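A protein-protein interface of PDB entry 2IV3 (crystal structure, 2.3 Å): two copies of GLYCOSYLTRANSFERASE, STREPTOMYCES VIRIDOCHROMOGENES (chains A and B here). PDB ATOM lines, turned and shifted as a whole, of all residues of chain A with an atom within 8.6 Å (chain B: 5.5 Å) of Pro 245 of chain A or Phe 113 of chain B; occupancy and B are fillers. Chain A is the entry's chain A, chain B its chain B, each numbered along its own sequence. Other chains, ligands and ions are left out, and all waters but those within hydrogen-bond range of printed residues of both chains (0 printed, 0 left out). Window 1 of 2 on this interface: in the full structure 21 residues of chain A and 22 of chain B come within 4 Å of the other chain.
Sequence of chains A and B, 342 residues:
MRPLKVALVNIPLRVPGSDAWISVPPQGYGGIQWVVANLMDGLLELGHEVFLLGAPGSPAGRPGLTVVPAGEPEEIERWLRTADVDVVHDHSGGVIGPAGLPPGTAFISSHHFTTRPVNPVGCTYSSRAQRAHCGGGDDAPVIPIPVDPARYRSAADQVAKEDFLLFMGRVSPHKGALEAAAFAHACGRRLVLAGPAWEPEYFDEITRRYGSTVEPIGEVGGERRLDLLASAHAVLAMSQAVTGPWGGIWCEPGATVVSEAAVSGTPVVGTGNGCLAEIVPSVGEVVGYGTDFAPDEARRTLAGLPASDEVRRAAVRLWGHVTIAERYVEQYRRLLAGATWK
Thr 115 of chain A touches Thr 115 of chain B (OG1 to CG2, 3.2 Å).
OG1 of Thr 243 of chain A touches CG1 of Ile 11 of chain B (3.8 Å).
CG2 of Thr 243 of chain A touches CD1 of Leu 13 of chain B (3.8 Å).
CD1 of Ile 11 of chain B touches O of Gly 244 of chain A, at 3.8 Å.
Pro 245 of chain A touches Phe 113 of chain B.
O of Trp 246 of chain A touches CG of Phe 113 of chain B, at 3.8 Å.
Gly 93 of chain B touches Gly 247 of chain A (O to C, 3.9 Å).
Gly 247 of chain A touches Phe 113 of chain B (CA to CZ, 3.5 Å).
N of Gly 248 of chain A touches O of Ser 92 of chain B, 3.5 Å away.
Gly 248 of chain A touches Gly 93 of chain B (N to O, 3.7 Å).
Hydrophobic or aromatic side chains of chain B within 4 Å of the printed part of chain A: Ile 11, Leu 13 and Phe 113.
Among the printed residues, 11 pairs touch across the chains.
Among the printed residues, no Asp or Glu carboxylate lies within 4 Å of a Lys or Arg side-chain nitrogen of the other chain.
Thr 115 of chain B touches its own counterpart, Thr 115 of chain A.
2 positions are printed for both chains.
Of the 11 pairs that touch across the chains among the printed residues, 1 has its exchanged pair printed and touching as well.
His 174 of chain A touches none of the printed residues of chain B.
Of the printed residues of chain B, Gly 244 of chain A touches Ile 11 (3.8 Å).
Of chain B, only Phe 113 comes within 4 Å of Pro 245 of chain A.
No residue of chain A comes within 4 Å of Thr 114 of chain B.
Printed residues of chain A within 4 Å of Thr 115 of chain B: Thr 115 (3.2 Å) and Trp 246 (3.3 Å).
The nearest residue of chain A that does not touch Phe 113 of chain B is Gly 244 of chain A (4.4 Å).
The backbone carbonyl oxygen (O) of Trp 246 of chain A is in hydrogen-bond range of the side-chain hydroxyl (OG1) of Thr 115 of chain B, 3.3 Å away.
The indole nitrogen (NE1) of Trp 246 of chain A lies within hydrogen-bond range of the backbone carbonyl oxygen (O) of Gly 248 of chain A (3.4 Å).
NE2 of His 111 of chain B lies within hydrogen-bond range of O of Phe 113 of chain B.
O of Thr 115 of chain B sits at hydrogen-bond distance from NE2 of His 111 of chain B, 2.6 Å away.
NE2 of Gln 130 of chain B sits at hydrogen-bond distance from O of Phe 113 of chain B, at 3.4 Å.
The backbone carbonyl oxygen of Phe 113 of chain B is in hydrogen-bond range of the side-chain sulfur of Cys 134 of chain B (3.8 Å).
The backbone carbonyl oxygen of Thr 115 of chain B sits at hydrogen-bond distance from the side-chain sulfur of Cys 134 of chain B (3.4 Å).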
ATOM      1  N   THR A 114     -21.710 -22.474 -18.195  1.00  0.00           N
ATOM      2  CA  THR A 114     -21.021 -21.520 -19.061  1.00  0.00           C
ATOM      3  C   THR A 114     -19.676 -22.069 -19.473  1.00  0.00           C
ATOM      4  O   THR A 114     -19.036 -21.589 -20.421  1.00  0.00           O
ATOM      5  CB  THR A 114     -20.908 -20.205 -18.317  1.00  0.00           C
ATOM      6  OG1 THR A 114     -21.834 -19.284 -18.888  1.00  0.00           O
ATOM      7  CG2 THR A 114     -19.514 -19.596 -18.370  1.00  0.00           C
ATOM      8  N   THR A 115     -19.253 -23.108 -18.757  1.00  0.00           N
ATOM      9  CA  THR A 115     -17.887 -23.566 -18.837  1.00  0.00           C
ATOM     10  C   THR A 115     -17.862 -24.865 -19.547  1.00  0.00           C
ATOM     11  O   THR A 115     -18.881 -25.539 -19.650  1.00  0.00           O
ATOM     12  CB  THR A 115     -17.296 -23.722 -17.442  1.00  0.00           C
ATOM     13  OG1 THR A 115     -18.132 -24.586 -16.656  1.00  0.00           O
ATOM     14  CG2 THR A 115     -17.236 -22.358 -16.758  1.00  0.00           C
ATOM     15  N   PRO A 173     -24.833  -9.625 -10.858  1.00  0.00           N
ATOM     16  CA  PRO A 173     -24.508  -8.762 -11.979  1.00  0.00           C
ATOM     17  C   PRO A 173     -24.672  -9.392 -13.361  1.00  0.00           C
ATOM     18  O   PRO A 173     -25.182  -8.729 -14.264  1.00  0.00           O
ATOM     19  CB  PRO A 173     -23.039  -8.394 -11.714  1.00  0.00           C
ATOM     20  CG  PRO A 173     -22.888  -8.539 -10.239  1.00  0.00           C
ATOM     21  CD  PRO A 173     -23.665  -9.785  -9.976  1.00  0.00           C
ATOM     22  N   HIS A 174     -24.263 -10.642 -13.527  1.00  0.00           N
ATOM     23  CA  HIS A 174     -24.309 -11.259 -14.837  1.00  0.00           C
ATOM     24  C   HIS A 174     -25.734 -11.613 -15.260  1.00  0.00           C
ATOM     25  O   HIS A 174     -25.931 -12.025 -16.404  1.00  0.00           O
ATOM     26  CB  HIS A 174     -23.428 -12.513 -14.900  1.00  0.00           C
ATOM     27  CG  HIS A 174     -23.866 -13.592 -13.962  1.00  0.00           C
ATOM     28  ND1 HIS A 174     -23.487 -13.624 -12.638  1.00  0.00           N
ATOM     29  CD2 HIS A 174     -24.667 -14.667 -14.147  1.00  0.00           C
ATOM     30  CE1 HIS A 174     -24.022 -14.676 -12.049  1.00  0.00           C
ATOM     31  NE2 HIS A 174     -24.757 -15.313 -12.937  1.00  0.00           N
ATOM     32  N   GLU A 199     -25.692 -10.842  -2.927  1.00  0.00           N
ATOM     33  CA  GLU A 199     -24.631  -9.866  -3.065  1.00  0.00           C
ATOM     34  C   GLU A 199     -25.168  -8.502  -2.656  1.00  0.00           C
ATOM     35  O   GLU A 199     -25.928  -7.877  -3.411  1.00  0.00           O
ATOM     36  CB  GLU A 199     -24.164  -9.882  -4.506  1.00  0.00           C
ATOM     37  CG  GLU A 199     -24.085 -11.321  -5.037  1.00  0.00           C
ATOM     38  CD  GLU A 199     -23.495 -11.421  -6.398  1.00  0.00           C
ATOM     39  OE1 GLU A 199     -22.765 -10.492  -6.801  1.00  0.00           O
ATOM     40  OE2 GLU A 199     -23.754 -12.444  -7.076  1.00  0.00           O
ATOM     41  N   VAL A 242     -20.521  -9.978 -18.930  1.00  0.00           N
ATOM     42  CA  VAL A 242     -19.628  -9.476 -17.905  1.00  0.00           C
ATOM     43  C   VAL A 242     -18.729 -10.619 -17.492  1.00  0.00           C
ATOM     44  O   VAL A 242     -19.028 -11.807 -17.719  1.00  0.00           O
ATOM     45  CB  VAL A 242     -20.383  -8.890 -16.645  1.00  0.00           C
ATOM     46  CG1 VAL A 242     -21.164  -7.640 -16.994  1.00  0.00           C
ATOM     47  CG2 VAL A 242     -21.288  -9.934 -15.991  1.00  0.00           C
ATOM     48  N   THR A 243     -17.615 -10.245 -16.902  1.00  0.00           N
ATOM     49  CA  THR A 243     -16.623 -11.187 -16.474  1.00  0.00           C
ATOM     50  C   THR A 243     -17.068 -11.850 -15.195  1.00  0.00           C
ATOM     51  O   THR A 243     -17.728 -11.223 -14.374  1.00  0.00           O
ATOM     52  CB  THR A 243     -15.314 -10.461 -16.219  1.00  0.00           C
ATOM     53  OG1 THR A 243     -14.469 -11.300 -15.427  1.00  0.00           O
ATOM     54  CG2 THR A 243     -15.574  -9.184 -15.463  1.00  0.00           C
ATOM     55  N   GLY A 244     -16.693 -13.108 -14.995  1.00  0.00           N
ATOM     56  CA  GLY A 244     -16.986 -13.720 -13.695  1.00  0.00           C
ATOM     57  C   GLY A 244     -16.086 -14.708 -12.975  1.00  0.00           C
ATOM     58  O   GLY A 244     -15.106 -15.228 -13.539  1.00  0.00           O
ATOM     59  N   PRO A 245     -16.446 -14.978 -11.695  1.00  0.00           N
ATOM     60  CA  PRO A 245     -15.983 -16.080 -10.827  1.00  0.00           C
ATOM     61  C   PRO A 245     -15.937 -17.452 -11.515  1.00  0.00           C
ATOM     62  O   PRO A 245     -15.045 -18.229 -11.227  1.00  0.00           O
ATOM     63  CB  PRO A 245     -17.031 -16.088  -9.696  1.00  0.00           C
ATOM     64  CG  PRO A 245     -17.411 -14.644  -9.555  1.00  0.00           C
ATOM     65  CD  PRO A 245     -17.408 -14.099 -10.987  1.00  0.00           C
ATOM     66  N   TRP A 246     -16.865 -17.765 -12.406  1.00  0.00           N
ATOM     67  CA  TRP A 246     -16.748 -19.022 -13.187  1.00  0.00           C
ATOM     68  C   TRP A 246     -15.477 -18.970 -14.029  1.00  0.00           C
ATOM     69  O   TRP A 246     -15.004 -20.015 -14.460  1.00  0.00           O
ATOM     70  CB  TRP A 246     -17.940 -19.194 -14.132  1.00  0.00           C
ATOM     71  CG  TRP A 246     -18.252 -17.881 -14.741  1.00  0.00           C
ATOM     72  CD1 TRP A 246     -17.793 -17.390 -15.932  1.00  0.00           C
ATOM     73  CD2 TRP A 246     -19.006 -16.825 -14.126  1.00  0.00           C
ATOM     74  NE1 TRP A 246     -18.228 -16.091 -16.100  1.00  0.00           N
ATOM     75  CE2 TRP A 246     -18.976 -15.724 -15.006  1.00  0.00           C
ATOM     76  CE3 TRP A 246     -19.710 -16.711 -12.916  1.00  0.00           C
ATOM     77  CZ2 TRP A 246     -19.640 -14.531 -14.724  1.00  0.00           C
ATOM     78  CZ3 TRP A 246     -20.340 -15.525 -12.632  1.00  0.00           C
ATOM     79  CH2 TRP A 246     -20.307 -14.449 -13.538  1.00  0.00           C
ATOM     80  N   GLY A 247     -14.951 -17.757 -14.268  1.00  0.00           N
ATOM     81  CA  GLY A 247     -13.858 -17.531 -15.229  1.00  0.00           C
ATOM     82  C   GLY A 247     -14.268 -17.384 -16.698  1.00  0.00           C
ATOM     83  O   GLY A 247     -14.870 -18.305 -17.276  1.00  0.00           O
ATOM     84  N   GLY A 248     -13.917 -16.239 -17.305  1.00  0.00           N
ATOM     85  CA  GLY A 248     -14.334 -15.895 -18.670  1.00  0.00           C
ATOM     86  C   GLY A 248     -15.451 -14.859 -18.672  1.00  0.00           C
ATOM     87  O   GLY A 248     -15.805 -14.302 -17.608  1.00  0.00           O
ATOM     88  N   ILE A 249     -15.997 -14.574 -19.860  1.00  0.00           N
ATOM     89  CA  ILE A 249     -17.181 -13.696 -20.012  1.00  0.00           C
ATOM     90  C   ILE A 249     -18.470 -14.525 -19.858  1.00  0.00           C
ATOM     91  O   ILE A 249     -18.544 -15.669 -20.315  1.00  0.00           O
ATOM     92  CB  ILE A 249     -17.209 -12.996 -21.407  1.00  0.00           C
ATOM     93  CG1 ILE A 249     -15.914 -12.256 -21.711  1.00  0.00           C
ATOM     94  CG2 ILE A 249     -18.386 -12.072 -21.520  1.00  0.00           C
ATOM     95  CD1 ILE A 249     -15.637 -11.010 -20.836  1.00  0.00           C
ATOM     96  N   TRP A 250     -19.488 -13.956 -19.228  1.00  0.00           N
ATOM     97  CA  TRP A 250     -20.730 -14.685 -19.015  1.00  0.00           C
ATOM     98  C   TRP A 250     -21.499 -14.891 -20.326  1.00  0.00           C
ATOM     99  O   TRP A 250     -21.539 -14.032 -21.213  1.00  0.00           O
ATOM    100  CB  TRP A 250     -21.590 -14.018 -17.936  1.00  0.00           C
ATOM    101  CG  TRP A 250     -22.932 -14.704 -17.755  1.00  0.00           C
ATOM    102  CD1 TRP A 250     -24.117 -14.291 -18.250  1.00  0.00           C
ATOM    103  CD2 TRP A 250     -23.189 -15.931 -17.069  1.00  0.00           C
ATOM    104  NE1 TRP A 250     -25.099 -15.184 -17.937  1.00  0.00           N
ATOM    105  CE2 TRP A 250     -24.558 -16.197 -17.196  1.00  0.00           C
ATOM    106  CE3 TRP A 250     -22.389 -16.838 -16.365  1.00  0.00           C
ATOM    107  CZ2 TRP A 250     -25.161 -17.326 -16.636  1.00  0.00           C
ATOM    108  CZ3 TRP A 250     -22.985 -17.945 -15.801  1.00  0.00           C
ATOM    109  CH2 TRP A 250     -24.357 -18.188 -15.951  1.00  0.00           C
ATOM    110  N   ILE B  11      -7.924 -10.786 -14.124  1.00  0.00           N
ATOM    111  CA  ILE B  11      -9.367 -10.902 -14.215  1.00  0.00           C
ATOM    112  C   ILE B  11     -10.056  -9.550 -14.033  1.00  0.00           C
ATOM    113  O   ILE B  11     -10.016  -8.975 -12.919  1.00  0.00           O
ATOM    114  CB  ILE B  11      -9.923 -11.926 -13.181  1.00  0.00           C
ATOM    115  CG1 ILE B  11     -11.438 -12.066 -13.343  1.00  0.00           C
ATOM    116  CG2 ILE B  11      -9.507 -11.570 -11.724  1.00  0.00           C
ATOM    117  CD1 ILE B  11     -12.015 -13.197 -12.630  1.00  0.00           C
ATOM    118  N   LEU B  13     -12.543  -6.937 -13.116  1.00  0.00           N
ATOM    119  CA  LEU B  13     -13.555  -7.069 -12.076  1.00  0.00           C
ATOM    120  C   LEU B  13     -13.850  -5.759 -11.347  1.00  0.00           C
ATOM    121  O   LEU B  13     -12.935  -5.099 -10.877  1.00  0.00           O
ATOM    122  CB  LEU B  13     -13.023  -8.078 -11.061  1.00  0.00           C
ATOM    123  CG  LEU B  13     -13.882  -9.255 -10.663  1.00  0.00           C
ATOM    124  CD1 LEU B  13     -14.920  -9.568 -11.741  1.00  0.00           C
ATOM    125  CD2 LEU B  13     -12.951 -10.447 -10.375  1.00  0.00           C
ATOM    126  N   ILE B  32      -6.838 -14.222  -7.363  1.00  0.00           N
ATOM    127  CA  ILE B  32      -6.125 -14.090  -8.658  1.00  0.00           C
ATOM    128  C   ILE B  32      -5.332 -12.780  -8.782  1.00  0.00           C
ATOM    129  O   ILE B  32      -4.285 -12.732  -9.458  1.00  0.00           O
ATOM    130  CB  ILE B  32      -7.081 -14.086  -9.857  1.00  0.00           C
ATOM    131  CG1 ILE B  32      -7.935 -15.380  -9.880  1.00  0.00           C
ATOM    132  CG2 ILE B  32      -6.257 -13.772 -11.178  1.00  0.00           C
ATOM    133  CD1 ILE B  32      -9.021 -15.410 -10.935  1.00  0.00           C
ATOM    134  N   HIS B  91      -4.577 -14.316 -17.014  1.00  0.00           N
ATOM    135  CA  HIS B  91      -4.979 -14.801 -15.713  1.00  0.00           C
ATOM    136  C   HIS B  91      -6.465 -14.687 -15.529  1.00  0.00           C
ATOM    137  O   HIS B  91      -6.975 -15.048 -14.492  1.00  0.00           O
ATOM    138  CB  HIS B  91      -4.290 -13.971 -14.640  1.00  0.00           C
ATOM    139  CG  HIS B  91      -2.864 -14.343 -14.437  1.00  0.00           C
ATOM    140  ND1 HIS B  91      -1.840 -13.748 -15.138  1.00  0.00           N
ATOM    141  CD2 HIS B  91      -2.294 -15.273 -13.643  1.00  0.00           C
ATOM    142  CE1 HIS B  91      -0.692 -14.290 -14.782  1.00  0.00           C
ATOM    143  NE2 HIS B  91      -0.938 -15.214 -13.870  1.00  0.00           N
ATOM    144  N   SER B  92      -7.150 -14.168 -16.540  1.00  0.00           N
ATOM    145  CA  SER B  92      -8.593 -13.851 -16.450  1.00  0.00           C
ATOM    146  C   SER B  92      -9.517 -15.031 -16.727  1.00  0.00           C
ATOM    147  O   SER B  92     -10.742 -14.940 -16.488  1.00  0.00           O
ATOM    148  CB  SER B  92      -8.958 -12.723 -17.410  1.00  0.00           C
ATOM    149  OG  SER B  92      -8.817 -13.190 -18.738  1.00  0.00           O
ATOM    150  N   GLY B  93      -8.954 -16.114 -17.259  1.00  0.00           N
ATOM    151  CA  GLY B  93      -9.738 -17.326 -17.512  1.00  0.00           C
ATOM    152  C   GLY B  93     -10.412 -17.329 -18.862  1.00  0.00           C
ATOM    153  O   GLY B  93     -11.303 -18.147 -19.123  1.00  0.00           O
ATOM    154  N   HIS B 111      -4.206 -21.002 -15.166  1.00  0.00           N
ATOM    155  CA  HIS B 111      -5.592 -21.382 -14.902  1.00  0.00           C
ATOM    156  C   HIS B 111      -6.014 -21.365 -13.409  1.00  0.00           C
ATOM    157  O   HIS B 111      -5.539 -22.174 -12.646  1.00  0.00           O
ATOM    158  CB  HIS B 111      -5.853 -22.745 -15.539  1.00  0.00           C
ATOM    159  CG  HIS B 111      -7.296 -23.089 -15.608  1.00  0.00           C
ATOM    160  ND1 HIS B 111      -8.232 -22.241 -16.159  1.00  0.00           N
ATOM    161  CD2 HIS B 111      -7.973 -24.181 -15.180  1.00  0.00           C
ATOM    162  CE1 HIS B 111      -9.422 -22.796 -16.070  1.00  0.00           C
ATOM    163  NE2 HIS B 111      -9.290 -23.973 -15.482  1.00  0.00           N
ATOM    164  N   HIS B 112      -6.876 -20.451 -12.991  1.00  0.00           N
ATOM    165  CA  HIS B 112      -7.285 -20.346 -11.579  1.00  0.00           C
ATOM    166  C   HIS B 112      -8.678 -20.878 -11.189  1.00  0.00           C
ATOM    167  O   HIS B 112      -9.205 -20.543 -10.124  1.00  0.00           O
ATOM    168  CB  HIS B 112      -7.196 -18.898 -11.120  1.00  0.00           C
ATOM    169  CG  HIS B 112      -5.918 -18.211 -11.502  1.00  0.00           C
ATOM    170  ND1 HIS B 112      -5.815 -17.394 -12.614  1.00  0.00           N
ATOM    171  CD2 HIS B 112      -4.692 -18.211 -10.915  1.00  0.00           C
ATOM    172  CE1 HIS B 112      -4.580 -16.924 -12.690  1.00  0.00           C
ATOM    173  NE2 HIS B 112      -3.883 -17.393 -11.668  1.00  0.00           N
ATOM    174  N   PHE B 113      -9.295 -21.702 -12.019  1.00  0.00           N
ATOM    175  CA  PHE B 113     -10.671 -22.161 -11.786  1.00  0.00           C
ATOM    176  C   PHE B 113     -10.776 -23.668 -11.748  1.00  0.00           C
ATOM    177  O   PHE B 113      -9.949 -24.376 -12.340  1.00  0.00           O
ATOM    178  CB  PHE B 113     -11.615 -21.588 -12.881  1.00  0.00           C
ATOM    179  CG  PHE B 113     -11.409 -20.134 -13.114  1.00  0.00           C
ATOM    180  CD1 PHE B 113     -11.946 -19.205 -12.250  1.00  0.00           C
ATOM    181  CD2 PHE B 113     -10.582 -19.694 -14.131  1.00  0.00           C
ATOM    182  CE1 PHE B 113     -11.711 -17.884 -12.434  1.00  0.00           C
ATOM    183  CE2 PHE B 113     -10.335 -18.351 -14.298  1.00  0.00           C
ATOM    184  CZ  PHE B 113     -10.892 -17.456 -13.440  1.00  0.00           C
ATOM    185  N   THR B 114     -11.839 -24.136 -11.099  1.00  0.00           N
ATOM    186  CA  THR B 114     -12.244 -25.553 -11.085  1.00  0.00           C
ATOM    187  C   THR B 114     -12.774 -26.117 -12.397  1.00  0.00           C
ATOM    188  O   THR B 114     -12.769 -27.345 -12.602  1.00  0.00           O
ATOM    189  CB  THR B 114     -13.276 -25.795 -10.027  1.00  0.00           C
ATOM    190  OG1 THR B 114     -14.369 -24.887 -10.203  1.00  0.00           O
ATOM    191  CG2 THR B 114     -12.654 -25.514  -8.728  1.00  0.00           C
ATOM    192  N   THR B 115     -13.194 -25.232 -13.303  1.00  0.00           N
ATOM    193  CA  THR B 115     -13.741 -25.636 -14.611  1.00  0.00           C
ATOM    194  C   THR B 115     -12.651 -25.765 -15.671  1.00  0.00           C
ATOM    195  O   THR B 115     -11.558 -25.245 -15.466  1.00  0.00           O
ATOM    196  CB  THR B 115     -14.826 -24.653 -15.025  1.00  0.00           C
ATOM    197  OG1 THR B 115     -14.454 -23.312 -14.630  1.00  0.00           O
ATOM    198  CG2 THR B 115     -16.103 -25.008 -14.276  1.00  0.00           C
ATOM    199  N   GLN B 130      -5.538 -30.061 -10.149  1.00  0.00           N
ATOM    200  CA  GLN B 130      -6.215 -29.185 -11.087  1.00  0.00           C
ATOM    201  C   GLN B 130      -6.054 -29.603 -12.557  1.00  0.00           C
ATOM    202  O   GLN B 130      -7.057 -29.822 -13.259  1.00  0.00           O
ATOM    203  CB  GLN B 130      -5.706 -27.765 -10.929  1.00  0.00           C
ATOM    204  CG  GLN B 130      -6.526 -26.750 -11.713  1.00  0.00           C
ATOM    205  CD  GLN B 130      -5.782 -25.476 -11.945  1.00  0.00           C
ATOM    206  OE1 GLN B 130      -4.575 -25.454 -11.878  1.00  0.00           O
ATOM    207  NE2 GLN B 130      -6.506 -24.399 -12.228  1.00  0.00           N
ATOM    208  N   CYS B 134      -9.278 -30.553 -14.842  1.00  0.00           N
ATOM    209  CA  CYS B 134      -9.656 -29.681 -15.957  1.00  0.00           C
ATOM    210  C   CYS B 134      -9.368 -30.303 -17.295  1.00  0.00           C
ATOM    211  O   CYS B 134      -9.645 -29.687 -18.320  1.00  0.00           O
ATOM    212  CB  CYS B 134      -8.879 -28.371 -15.885  1.00  0.00           C
ATOM    213  SG  CYS B 134      -9.235 -27.448 -14.444  1.00  0.00           S
ATOM    214  N   PRO B 253      -8.171 -25.250  -6.948  1.00  0.00           N
ATOM    215  CA  PRO B 253      -7.111 -25.067  -7.948  1.00  0.00           C
ATOM    216  C   PRO B 253      -5.692 -24.746  -7.411  1.00  0.00           C
ATOM    217  O   PRO B 253      -4.743 -25.459  -7.764  1.00  0.00           O
ATOM    218  CB  PRO B 253      -7.634 -23.907  -8.824  1.00  0.00           C
ATOM    219  CG  PRO B 253      -8.766 -23.302  -8.103  1.00  0.00           C
ATOM    220  CD  PRO B 253      -9.182 -24.170  -6.992  1.00  0.00           C
